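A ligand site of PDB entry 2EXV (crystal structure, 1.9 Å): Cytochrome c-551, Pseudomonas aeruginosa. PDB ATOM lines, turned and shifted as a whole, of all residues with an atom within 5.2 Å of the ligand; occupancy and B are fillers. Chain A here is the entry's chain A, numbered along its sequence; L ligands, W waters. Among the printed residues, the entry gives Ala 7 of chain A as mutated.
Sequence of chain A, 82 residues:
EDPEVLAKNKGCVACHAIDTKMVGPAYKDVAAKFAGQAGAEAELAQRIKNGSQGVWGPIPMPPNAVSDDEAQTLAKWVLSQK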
ATOM      1  N   ALA A   7      11.963  16.761 -19.287  1.00  0.00           N
ATOM      2  CA  ALA A   7      13.120  17.199 -18.479  1.00  0.00           C
ATOM      3  C   ALA A   7      14.354  16.372 -18.766  1.00  0.00           C
ATOM      4  O   ALA A   7      15.473  16.872 -18.785  1.00  0.00           O
ATOM      5  CB  ALA A   7      12.797  17.191 -16.967  1.00  0.00           C
ATOM      6  N   LYS A  10      15.288  16.820 -22.915  1.00  0.00           N
ATOM      7  CA  LYS A  10      15.752  18.158 -23.250  1.00  0.00           C
ATOM      8  C   LYS A  10      16.952  18.564 -22.396  1.00  0.00           C
ATOM      9  O   LYS A  10      17.399  19.698 -22.467  1.00  0.00           O
ATOM     10  CB  LYS A  10      14.606  19.146 -23.113  1.00  0.00           C
ATOM     11  CG  LYS A  10      13.467  18.905 -24.086  1.00  0.00           C
ATOM     12  CD  LYS A  10      13.930  19.176 -25.532  1.00  0.00           C
ATOM     13  CE  LYS A  10      12.811  19.001 -26.534  1.00  0.00           C
ATOM     14  NZ  LYS A  10      12.834  17.687 -27.226  1.00  0.00           N
ATOM     15  N   GLY A  11      17.494  17.621 -21.623  1.00  0.00           N
ATOM     16  CA  GLY A  11      18.762  17.857 -20.935  1.00  0.00           C
ATOM     17  C   GLY A  11      18.727  18.648 -19.638  1.00  0.00           C
ATOM     18  O   GLY A  11      19.767  18.910 -19.049  1.00  0.00           O
ATOM     19  N   CYS A  12      17.524  18.998 -19.175  1.00  0.00           N
ATOM     20  CA  CYS A  12      17.324  19.712 -17.886  1.00  0.00           C
ATOM     21  C   CYS A  12      17.915  18.952 -16.713  1.00  0.00           C
ATOM     22  O   CYS A  12      18.455  19.580 -15.794  1.00  0.00           O
ATOM     23  CB  CYS A  12      15.823  19.923 -17.625  1.00  0.00           C
ATOM     24  SG  CYS A  12      14.812  20.409 -19.060  1.00  0.00           S
ATOM     25  N   ALA A  14      20.627  17.427 -16.417  1.00  0.00           N
ATOM     26  CA  ALA A  14      22.078  17.621 -16.248  1.00  0.00           C
ATOM     27  C   ALA A  14      22.355  18.705 -15.214  1.00  0.00           C
ATOM     28  O   ALA A  14      23.395  18.672 -14.560  1.00  0.00           O
ATOM     29  CB  ALA A  14      22.724  17.957 -17.561  1.00  0.00           C
ATOM     30  N   CYS A  15      21.396  19.631 -15.050  1.00  0.00           N
ATOM     31  CA  CYS A  15      21.614  20.833 -14.247  1.00  0.00           C
ATOM     32  C   CYS A  15      20.559  21.087 -13.146  1.00  0.00           C
ATOM     33  O   CYS A  15      20.757  21.967 -12.307  1.00  0.00           O
ATOM     34  CB  CYS A  15      21.605  22.074 -15.168  1.00  0.00           C
ATOM     35  SG  CYS A  15      22.967  22.093 -16.337  1.00  0.00           S
ATOM     36  N   HIS A  16      19.470  20.307 -13.130  1.00  0.00           N
ATOM     37  CA  HIS A  16      18.393  20.563 -12.181  1.00  0.00           C
ATOM     38  C   HIS A  16      17.839  19.254 -11.658  1.00  0.00           C
ATOM     39  O   HIS A  16      17.728  18.285 -12.417  1.00  0.00           O
ATOM     40  CB  HIS A  16      17.197  21.244 -12.850  1.00  0.00           C
ATOM     41  CG  HIS A  16      17.403  22.675 -13.262  1.00  0.00           C
ATOM     42  ND1 HIS A  16      17.224  23.740 -12.397  1.00  0.00           N
ATOM     43  CD2 HIS A  16      17.648  23.221 -14.481  1.00  0.00           C
ATOM     44  CE1 HIS A  16      17.386  24.874 -13.065  1.00  0.00           C
ATOM     45  NE2 HIS A  16      17.634  24.585 -14.326  1.00  0.00           N
ATOM     46  N   VAL A  23      23.384  22.644 -10.387  1.00  0.00           N
ATOM     47  CA  VAL A  23      23.923  23.883 -10.975  1.00  0.00           C
ATOM     48  C   VAL A  23      22.839  24.947 -10.925  1.00  0.00           C
ATOM     49  O   VAL A  23      23.090  26.129 -10.534  1.00  0.00           O
ATOM     50  CB  VAL A  23      24.283  23.723 -12.472  1.00  0.00           C
ATOM     51  CG1 VAL A  23      25.147  24.905 -12.883  1.00  0.00           C
ATOM     52  CG2 VAL A  23      24.975  22.412 -12.729  1.00  0.00           C
ATOM     53  N   GLY A  24      21.672  24.534 -11.386  1.00  0.00           N
ATOM     54  CA  GLY A  24      20.463  25.352 -11.400  1.00  0.00           C
ATOM     55  C   GLY A  24      19.702  25.127 -10.110  1.00  0.00           C
ATOM     56  O   GLY A  24      19.955  24.125  -9.435  1.00  0.00           O
ATOM     57  N   PRO A  25      18.761  26.036  -9.767  1.00  0.00           N
ATOM     58  CA  PRO A  25      18.014  25.835  -8.531  1.00  0.00           C
ATOM     59  C   PRO A  25      17.139  24.570  -8.585  1.00  0.00           C
ATOM     60  O   PRO A  25      16.705  24.177  -9.668  1.00  0.00           O
ATOM     61  CB  PRO A  25      17.114  27.077  -8.434  1.00  0.00           C
ATOM     62  CG  PRO A  25      17.034  27.651  -9.835  1.00  0.00           C
ATOM     63  CD  PRO A  25      18.325  27.227 -10.536  1.00  0.00           C
ATOM     64  N   TYR A  27      13.761  22.522  -8.448  1.00  0.00           N
ATOM     65  CA  TYR A  27      12.463  22.959  -8.922  1.00  0.00           C
ATOM     66  C   TYR A  27      11.543  23.279  -7.752  1.00  0.00           C
ATOM     67  O   TYR A  27      10.751  24.205  -7.818  1.00  0.00           O
ATOM     68  CB  TYR A  27      11.821  21.906  -9.829  1.00  0.00           C
ATOM     69  CG  TYR A  27      12.549  21.647 -11.155  1.00  0.00           C
ATOM     70  CD1 TYR A  27      12.626  20.355 -11.665  1.00  0.00           C
ATOM     71  CD2 TYR A  27      13.152  22.666 -11.881  1.00  0.00           C
ATOM     72  CE1 TYR A  27      13.267  20.092 -12.877  1.00  0.00           C
ATOM     73  CE2 TYR A  27      13.825  22.418 -13.116  1.00  0.00           C
ATOM     74  CZ  TYR A  27      13.855  21.107 -13.596  1.00  0.00           C
ATOM     75  OH  TYR A  27      14.518  20.820 -14.762  1.00  0.00           O
ATOM     76  N   VAL A  30      12.321  26.826  -6.829  1.00  0.00           N
ATOM     77  CA  VAL A  30      11.721  27.721  -7.811  1.00  0.00           C
ATOM     78  C   VAL A  30      10.221  27.933  -7.550  1.00  0.00           C
ATOM     79  O   VAL A  30       9.752  29.093  -7.496  1.00  0.00           O
ATOM     80  CB  VAL A  30      11.967  27.246  -9.247  1.00  0.00           C
ATOM     81  CG1 VAL A  30      11.290  28.184 -10.286  1.00  0.00           C
ATOM     82  CG2 VAL A  30      13.479  27.165  -9.525  1.00  0.00           C
ATOM     83  N   PHE A  34       8.498  31.557  -6.645  1.00  0.00           N
ATOM     84  CA  PHE A  34       7.600  32.225  -7.567  1.00  0.00           C
ATOM     85  C   PHE A  34       6.147  32.005  -7.196  1.00  0.00           C
ATOM     86  O   PHE A  34       5.247  32.462  -7.914  1.00  0.00           O
ATOM     87  CB  PHE A  34       7.881  31.773  -8.997  1.00  0.00           C
ATOM     88  CG  PHE A  34       9.198  32.265  -9.536  1.00  0.00           C
ATOM     89  CD1 PHE A  34      10.397  31.670  -9.153  1.00  0.00           C
ATOM     90  CD2 PHE A  34       9.229  33.359 -10.407  1.00  0.00           C
ATOM     91  CE1 PHE A  34      11.625  32.143  -9.623  1.00  0.00           C
ATOM     92  CE2 PHE A  34      10.467  33.835 -10.896  1.00  0.00           C
ATOM     93  CZ  PHE A  34      11.656  33.220 -10.492  1.00  0.00           C
ATOM     94  N   LEU A  44       8.604  32.139 -16.556  1.00  0.00           N
ATOM     95  CA  LEU A  44       9.465  30.976 -16.451  1.00  0.00           C
ATOM     96  C   LEU A  44       9.537  30.290 -17.789  1.00  0.00           C
ATOM     97  O   LEU A  44      10.590  29.827 -18.164  1.00  0.00           O
ATOM     98  CB  LEU A  44       8.977  29.979 -15.406  1.00  0.00           C
ATOM     99  CG  LEU A  44       9.174  30.185 -13.908  1.00  0.00           C
ATOM    100  CD1 LEU A  44       9.040  28.808 -13.223  1.00  0.00           C
ATOM    101  CD2 LEU A  44      10.530  30.814 -13.599  1.00  0.00           C
ATOM    102  N   ARG A  47      12.077  32.122 -19.917  1.00  0.00           N
ATOM    103  CA  ARG A  47      13.432  31.925 -19.403  1.00  0.00           C
ATOM    104  C   ARG A  47      13.968  30.519 -19.679  1.00  0.00           C
ATOM    105  O   ARG A  47      15.151  30.345 -19.965  1.00  0.00           O
ATOM    106  CB  ARG A  47      13.490  32.244 -17.919  1.00  0.00           C
ATOM    107  CG  ARG A  47      13.485  33.747 -17.650  1.00  0.00           C
ATOM    108  CD  ARG A  47      13.373  34.059 -16.170  1.00  0.00           C
ATOM    109  NE  ARG A  47      13.569  35.489 -15.925  1.00  0.00           N
ATOM    110  CZ  ARG A  47      13.247  36.126 -14.801  1.00  0.00           C
ATOM    111  NH1 ARG A  47      12.705  35.459 -13.787  1.00  0.00           N
ATOM    112  NH2 ARG A  47      13.487  37.437 -14.687  1.00  0.00           N
ATOM    113  N   ILE A  48      13.098  29.515 -19.574  1.00  0.00           N
ATOM    114  CA  ILE A  48      13.500  28.136 -19.912  1.00  0.00           C
ATOM    115  C   ILE A  48      13.916  28.064 -21.385  1.00  0.00           C
ATOM    116  O   ILE A  48      14.912  27.425 -21.729  1.00  0.00           O
ATOM    117  CB  ILE A  48      12.355  27.132 -19.615  1.00  0.00           C
ATOM    118  CG1 ILE A  48      12.205  26.939 -18.090  1.00  0.00           C
ATOM    119  CG2 ILE A  48      12.628  25.749 -20.321  1.00  0.00           C
ATOM    120  CD1 ILE A  48      10.826  26.331 -17.684  1.00  0.00           C
ATOM    121  N   SER A  52      18.631  32.505 -18.924  1.00  0.00           N
ATOM    122  CA  SER A  52      18.662  33.702 -18.059  1.00  0.00           C
ATOM    123  C   SER A  52      19.998  33.726 -17.319  1.00  0.00           C
ATOM    124  O   SER A  52      20.742  32.742 -17.327  1.00  0.00           O
ATOM    125  CB  SER A  52      17.492  33.671 -17.054  1.00  0.00           C
ATOM    126  OG  SER A  52      17.750  32.740 -16.026  1.00  0.00           O
ATOM    127  N   GLN A  53      20.274  34.842 -16.649  1.00  0.00           N
ATOM    128  CA  GLN A  53      21.414  34.917 -15.771  1.00  0.00           C
ATOM    129  C   GLN A  53      21.081  36.013 -14.760  1.00  0.00           C
ATOM    130  O   GLN A  53      20.540  37.073 -15.143  1.00  0.00           O
ATOM    131  CB  GLN A  53      22.662  35.274 -16.568  1.00  0.00           C
ATOM    132  CG  GLN A  53      23.939  35.461 -15.734  1.00  0.00           C
ATOM    133  CD  GLN A  53      25.173  35.778 -16.591  1.00  0.00           C
ATOM    134  OE1 GLN A  53      25.064  36.127 -17.753  1.00  0.00           O
ATOM    135  NE2 GLN A  53      26.354  35.635 -16.003  1.00  0.00           N
ATOM    136  N   GLY A  54      21.392  35.779 -13.493  1.00  0.00           N
ATOM    137  CA  GLY A  54      21.205  36.802 -12.468  1.00  0.00           C
ATOM    138  C   GLY A  54      19.820  36.746 -11.832  1.00  0.00           C
ATOM    139  O   GLY A  54      19.501  37.619 -11.015  1.00  0.00           O
ATOM    140  N   VAL A  55      19.004  35.745 -12.180  1.00  0.00           N
ATOM    141  CA  VAL A  55      17.692  35.574 -11.518  1.00  0.00           C
ATOM    142  C   VAL A  55      17.940  34.897 -10.162  1.00  0.00           C
ATOM    143  O   VAL A  55      17.439  35.329  -9.123  1.00  0.00           O
ATOM    144  CB  VAL A  55      16.696  34.720 -12.364  1.00  0.00           C
ATOM    145  CG1 VAL A  55      15.399  34.570 -11.595  1.00  0.00           C
ATOM    146  CG2 VAL A  55      16.454  35.414 -13.708  1.00  0.00           C
ATOM    147  N   TRP A  56      18.775  33.876 -10.212  1.00  0.00           N
ATOM    148  CA  TRP A  56      19.128  33.104  -9.023  1.00  0.00           C
ATOM    149  C   TRP A  56      20.589  33.248  -8.661  1.00  0.00           C
ATOM    150  O   TRP A  56      20.967  33.027  -7.515  1.00  0.00           O
ATOM    151  CB  TRP A  56      18.805  31.630  -9.289  1.00  0.00           C
ATOM    152  CG  TRP A  56      17.358  31.414  -9.273  1.00  0.00           C
ATOM    153  CD1 TRP A  56      16.493  31.593 -10.304  1.00  0.00           C
ATOM    154  CD2 TRP A  56      16.589  30.943  -8.181  1.00  0.00           C
ATOM    155  NE1 TRP A  56      15.223  31.281  -9.924  1.00  0.00           N
ATOM    156  CE2 TRP A  56      15.246  30.881  -8.607  1.00  0.00           C
ATOM    157  CE3 TRP A  56      16.897  30.586  -6.856  1.00  0.00           C
ATOM    158  CZ2 TRP A  56      14.205  30.451  -7.774  1.00  0.00           C
ATOM    159  CZ3 TRP A  56      15.871  30.173  -6.022  1.00  0.00           C
ATOM    160  CH2 TRP A  56      14.533  30.101  -6.488  1.00  0.00           C
ATOM    161  N   GLY A  57      21.395  33.662  -9.618  1.00  0.00           N
ATOM    162  CA  GLY A  57      22.824  33.893  -9.327  1.00  0.00           C
ATOM    163  C   GLY A  57      23.571  34.172 -10.601  1.00  0.00           C
ATOM    164  O   GLY A  57      22.944  34.352 -11.654  1.00  0.00           O
ATOM    165  N   PRO A  58      24.930  34.198 -10.516  1.00  0.00           N
ATOM    166  CA  PRO A  58      25.758  34.606 -11.636  1.00  0.00           C
ATOM    167  C   PRO A  58      25.911  33.541 -12.735  1.00  0.00           C
ATOM    168  O   PRO A  58      26.291  33.864 -13.875  1.00  0.00           O
ATOM    169  CB  PRO A  58      27.104  34.942 -10.973  1.00  0.00           C
ATOM    170  CG  PRO A  58      27.128  34.116  -9.735  1.00  0.00           C
ATOM    171  CD  PRO A  58      25.719  33.835  -9.322  1.00  0.00           C
ATOM    172  N   ILE A  59      25.607  32.284 -12.413  1.00  0.00           N
ATOM    173  CA  ILE A  59      25.753  31.214 -13.401  1.00  0.00           C
ATOM    174  C   ILE A  59      24.578  31.340 -14.368  1.00  0.00           C
ATOM    175  O   ILE A  59      23.435  31.402 -13.920  1.00  0.00           O
ATOM    176  CB  ILE A  59      25.723  29.800 -12.756  1.00  0.00           C
ATOM    177  CG1 ILE A  59      26.861  29.669 -11.728  1.00  0.00           C
ATOM    178  CG2 ILE A  59      25.844  28.704 -13.832  1.00  0.00           C
ATOM    179  CD1 ILE A  59      26.595  28.593 -10.707  1.00  0.00           C
ATOM    180  N   PRO A  60      24.861  31.411 -15.676  1.00  0.00           N
ATOM    181  CA  PRO A  60      23.745  31.511 -16.603  1.00  0.00           C
ATOM    182  C   PRO A  60      23.150  30.166 -16.951  1.00  0.00           C
ATOM    183  O   PRO A  60      23.868  29.146 -17.029  1.00  0.00           O
ATOM    184  CB  PRO A  60      24.382  32.115 -17.859  1.00  0.00           C
ATOM    185  CG  PRO A  60      25.808  31.929 -17.723  1.00  0.00           C
ATOM    186  CD  PRO A  60      26.147  31.381 -16.386  1.00  0.00           C
ATOM    187  N   MET A  61      21.836  30.161 -17.156  1.00  0.00           N
ATOM    188  CA  MET A  61      21.201  29.101 -17.904  1.00  0.00           C
ATOM    189  C   MET A  61      21.285  29.427 -19.398  1.00  0.00           C
ATOM    190  O   MET A  61      20.781  30.473 -19.841  1.00  0.00           O
ATOM    191  CB  MET A  61      19.746  28.948 -17.507  1.00  0.00           C
ATOM    192  CG  MET A  61      19.073  27.802 -18.309  1.00  0.00           C
ATOM    193  SD  MET A  61      17.500  27.189 -17.737  1.00  0.00           S
ATOM    194  CE  MET A  61      16.596  28.718 -17.572  1.00  0.00           C
ATOM    195  N   PRO A  62      21.900  28.535 -20.182  1.00  0.00           N
ATOM    196  CA  PRO A  62      21.910  28.825 -21.603  1.00  0.00           C
ATOM    197  C   PRO A  62      20.519  28.592 -22.179  1.00  0.00           C
ATOM    198  O   PRO A  62      19.714  27.913 -21.545  1.00  0.00           O
ATOM    199  CB  PRO A  62      22.846  27.742 -22.159  1.00  0.00           C
ATOM    200  CG  PRO A  62      23.629  27.284 -20.985  1.00  0.00           C
ATOM    201  CD  PRO A  62      22.601  27.279 -19.910  1.00  0.00           C
ATOM    202  N   ASN A  64      17.579  26.858 -24.105  1.00  0.00           N
ATOM    203  CA  ASN A  64      17.205  25.458 -24.348  1.00  0.00           C
ATOM    204  C   ASN A  64      16.395  25.266 -25.638  1.00  0.00           C
ATOM    205  O   ASN A  64      15.562  26.134 -25.998  1.00  0.00           O
ATOM    206  CB  ASN A  64      16.414  24.892 -23.161  1.00  0.00           C
ATOM    207  CG  ASN A  64      17.243  24.831 -21.895  1.00  0.00           C
ATOM    208  OD1 ASN A  64      18.128  23.985 -21.758  1.00  0.00           O
ATOM    209  ND2 ASN A  64      16.959  25.732 -20.964  1.00  0.00           N
ATOM    210  N   VAL A  66      13.778  24.052 -26.853  1.00  0.00           N
ATOM    211  CA  VAL A  66      12.392  23.663 -26.579  1.00  0.00           C
ATOM    212  C   VAL A  66      11.448  24.605 -27.330  1.00  0.00           C
ATOM    213  O   VAL A  66      11.768  25.784 -27.567  1.00  0.00           O
ATOM    214  CB  VAL A  66      12.053  23.645 -25.053  1.00  0.00           C
ATOM    215  CG1 VAL A  66      12.877  22.587 -24.280  1.00  0.00           C
ATOM    216  CG2 VAL A  66      12.211  25.035 -24.419  1.00  0.00           C
ATOM    217  N   LEU A  74       6.792  22.661 -19.252  1.00  0.00           N
ATOM    218  CA  LEU A  74       7.816  22.617 -18.215  1.00  0.00           C
ATOM    219  C   LEU A  74       7.589  23.622 -17.102  1.00  0.00           C
ATOM    220  O   LEU A  74       7.762  23.270 -15.944  1.00  0.00           O
ATOM    221  CB  LEU A  74       9.228  22.714 -18.835  1.00  0.00           C
ATOM    222  CG  LEU A  74       9.637  21.414 -19.590  1.00  0.00           C
ATOM    223  CD1 LEU A  74      10.746  21.693 -20.638  1.00  0.00           C
ATOM    224  CD2 LEU A  74      10.089  20.340 -18.592  1.00  0.00           C
ATOM    225  N   VAL A  78       7.082  22.824 -13.215  1.00  0.00           N
ATOM    226  CA  VAL A  78       8.034  23.320 -12.195  1.00  0.00           C
ATOM    227  C   VAL A  78       7.273  24.041 -11.089  1.00  0.00           C
ATOM    228  O   VAL A  78       7.519  23.799  -9.917  1.00  0.00           O
ATOM    229  CB  VAL A  78       9.107  24.230 -12.823  1.00  0.00           C
ATOM    230  CG1 VAL A  78       9.846  25.044 -11.712  1.00  0.00           C
ATOM    231  CG2 VAL A  78      10.133  23.367 -13.590  1.00  0.00           C
HETATM  232 FE1  LIG L   1      17.663  25.785 -15.913  1.00  0.00          FE
HETATM  233  C1  LIG L   1      17.271  28.511 -13.992  1.00  0.00           C
HETATM  234  C2  LIG L   1      14.292  25.161 -15.713  1.00  0.00           C
HETATM  235  C3  LIG L   1      17.955  23.374 -18.204  1.00  0.00           C
HETATM  236  C4  LIG L   1      21.083  25.839 -15.491  1.00  0.00           C
HETATM  237  N1  LIG L   1      16.056  26.694 -15.008  1.00  0.00           N
HETATM  238  C5  LIG L   1      16.113  27.821 -14.248  1.00  0.00           C
HETATM  239  C6  LIG L   1      14.785  28.143 -13.761  1.00  0.00           C
HETATM  240  C7  LIG L   1      13.960  27.187 -14.247  1.00  0.00           C
HETATM  241  C8  LIG L   1      14.759  26.259 -15.036  1.00  0.00           C
HETATM  242  C9  LIG L   1      12.445  27.039 -14.040  1.00  0.00           C
HETATM  243  C10 LIG L   1      14.446  29.352 -12.850  1.00  0.00           C
HETATM  244  C11 LIG L   1      14.236  30.642 -13.645  1.00  0.00           C
HETATM  245  C12 LIG L   1      15.537  31.276 -14.105  1.00  0.00           C
HETATM  246  O1  LIG L   1      15.684  31.505 -15.332  1.00  0.00           O
HETATM  247  O2  LIG L   1      16.407  31.537 -13.253  1.00  0.00           O
HETATM  248  N2  LIG L   1      16.324  24.525 -16.819  1.00  0.00           N
HETATM  249  C13 LIG L   1      14.987  24.425 -16.652  1.00  0.00           C
HETATM  250  C14 LIG L   1      14.432  23.515 -17.663  1.00  0.00           C
HETATM  251  C15 LIG L   1      15.480  22.999 -18.323  1.00  0.00           C
HETATM  252  C16 LIG L   1      16.661  23.650 -17.820  1.00  0.00           C
HETATM  253  C17 LIG L   1      12.942  23.095 -17.734  1.00  0.00           C
HETATM  254  C18 LIG L   1      15.551  21.994 -19.494  1.00  0.00           C
HETATM  255  C19 LIG L   1      14.717  22.473 -20.710  1.00  0.00           C
HETATM  256  N3  LIG L   1      19.227  24.796 -16.662  1.00  0.00           N
HETATM  257  C20 LIG L   1      19.111  23.850 -17.652  1.00  0.00           C
HETATM  258  C21 LIG L   1      20.474  23.516 -18.129  1.00  0.00           C
HETATM  259  C22 LIG L   1      21.356  24.109 -17.319  1.00  0.00           C
HETATM  260  C23 LIG L   1      20.567  24.955 -16.412  1.00  0.00           C
HETATM  261  C24 LIG L   1      20.710  22.380 -19.165  1.00  0.00           C
HETATM  262  C25 LIG L   1      22.904  23.859 -17.143  1.00  0.00           C
HETATM  263  C26 LIG L   1      23.709  24.395 -18.333  1.00  0.00           C
HETATM  264  N4  LIG L   1      18.948  26.952 -14.930  1.00  0.00           N
HETATM  265  C27 LIG L   1      20.329  26.811 -14.878  1.00  0.00           C
HETATM  266  C28 LIG L   1      20.874  27.877 -14.093  1.00  0.00           C
HETATM  267  C29 LIG L   1      19.711  28.690 -13.641  1.00  0.00           C
HETATM  268  C30 LIG L   1      18.551  28.051 -14.193  1.00  0.00           C
HETATM  269  C31 LIG L   1      22.354  28.135 -13.802  1.00  0.00           C
HETATM  270  C32 LIG L   1      19.749  29.975 -12.818  1.00  0.00           C
HETATM  271  C33 LIG L   1      19.842  31.076 -13.884  1.00  0.00           C
HETATM  272  C34 LIG L   1      19.795  32.454 -13.263  1.00  0.00           C
HETATM  273  O3  LIG L   1      20.267  32.660 -12.118  1.00  0.00           O
HETATM  274  O4  LIG L   1      19.333  33.417 -13.932  1.00  0.00           O
HETATM  275  O   HOH W   1      25.099  26.070 -16.086  1.00  0.00           O
HETATM  276  O   HOH W   2      22.650  31.244 -11.426  1.00  0.00           O
HETATM  277  O   HOH W   3      20.297  25.457 -20.948  1.00  0.00           O
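SG of Cys 12 is covalently linked to C18 of the ligand, 1.8 Å away. The side-chain sulfur of Cys 15 is bonded to a carbon (C25) of the ligand. NE2 of His 16 binds FE1 of the ligand, 2.0 Å away. An iron atom (FE1) of the ligand is bound by the side-chain sulfur (SD) of Met 61 (2.3 Å). The side-chain hydroxyl (OG) of Ser 52 is in hydrogen-bond range of an oxygen (O1) of the ligand, 2.5 Å away. The backbone NH (N) of Trp 56 sits at hydrogen-bond distance from an oxygen (O3) of the ligand (2.7 Å). The backbone NH (N) of Gly 57 sits at hydrogen-bond distance from an oxygen (O3) of the ligand, 2.9 Å away. An oxygen (O4) of the ligand is in hydrogen-bond range of the backbone NH of Val 55, at 2.9 Å. The backbone NH (N) of Gln 53 lies close to an oxygen (O4) of the ligand. N of Gly 54 sits at hydrogen-bond distance from O4 of the ligand (3.2 Å).
Residues that only touch the ligand: Gly 11, Val 23, Gly 24, Pro 25, Tyr 27, Leu 44, Arg 47, Ile 48, Ile 59, Pro 60, Pro 62, Asn 64 and Leu 74. Within 4 Å of the ligand: Gly 11, Cys 12, Cys 15, His 16, Val 23, Gly 24, Pro 25, Tyr 27, Leu 44, Arg 47, Ile 48, Ser 52, Gln 53, Gly 54, Val 55, Trp 56, Gly 57, Ile 59, Pro 60, Met 61, Pro 62, Asn 64 and Leu 74. The nearest printed residue that does not touch the ligand is Val 66 (4.02 Å).
Water W2 lies within hydrogen-bond range of O of Ile 59, O3 of the ligand and O of Gly 57. Water W3 lies within hydrogen-bond range of the backbone carbonyl oxygen of Pro 62 (2.6 Å) and the side-chain amide oxygen of Asn 64 (2.7 Å).
O of Ala 7 is in hydrogen-bond range of N of Cys 12 (3.0 Å). N of Gly 24 is in hydrogen-bond range of O of Cys 15, at 2.9 Å. The backbone carbonyl oxygen (O) of Cys 15 lies within hydrogen-bond range of the backbone NH (N) of Val 23 (3.3 Å). ND1 of His 16 sits at hydrogen-bond distance from O of Pro 25, at 2.8 Å. O of Ser 52 sits at hydrogen-bond distance from N of Met 61, 2.8 Å away. ND2 of Asn 64 sits close to SD of Met 61. The backbone carbonyl oxygen of Pro 58 lies within hydrogen-bond range of the side-chain amide nitrogen of Gln 53 (2.8 Å). O of Ile 48 lies within hydrogen-bond range of ND2 of Asn 64, at 2.8 Å.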
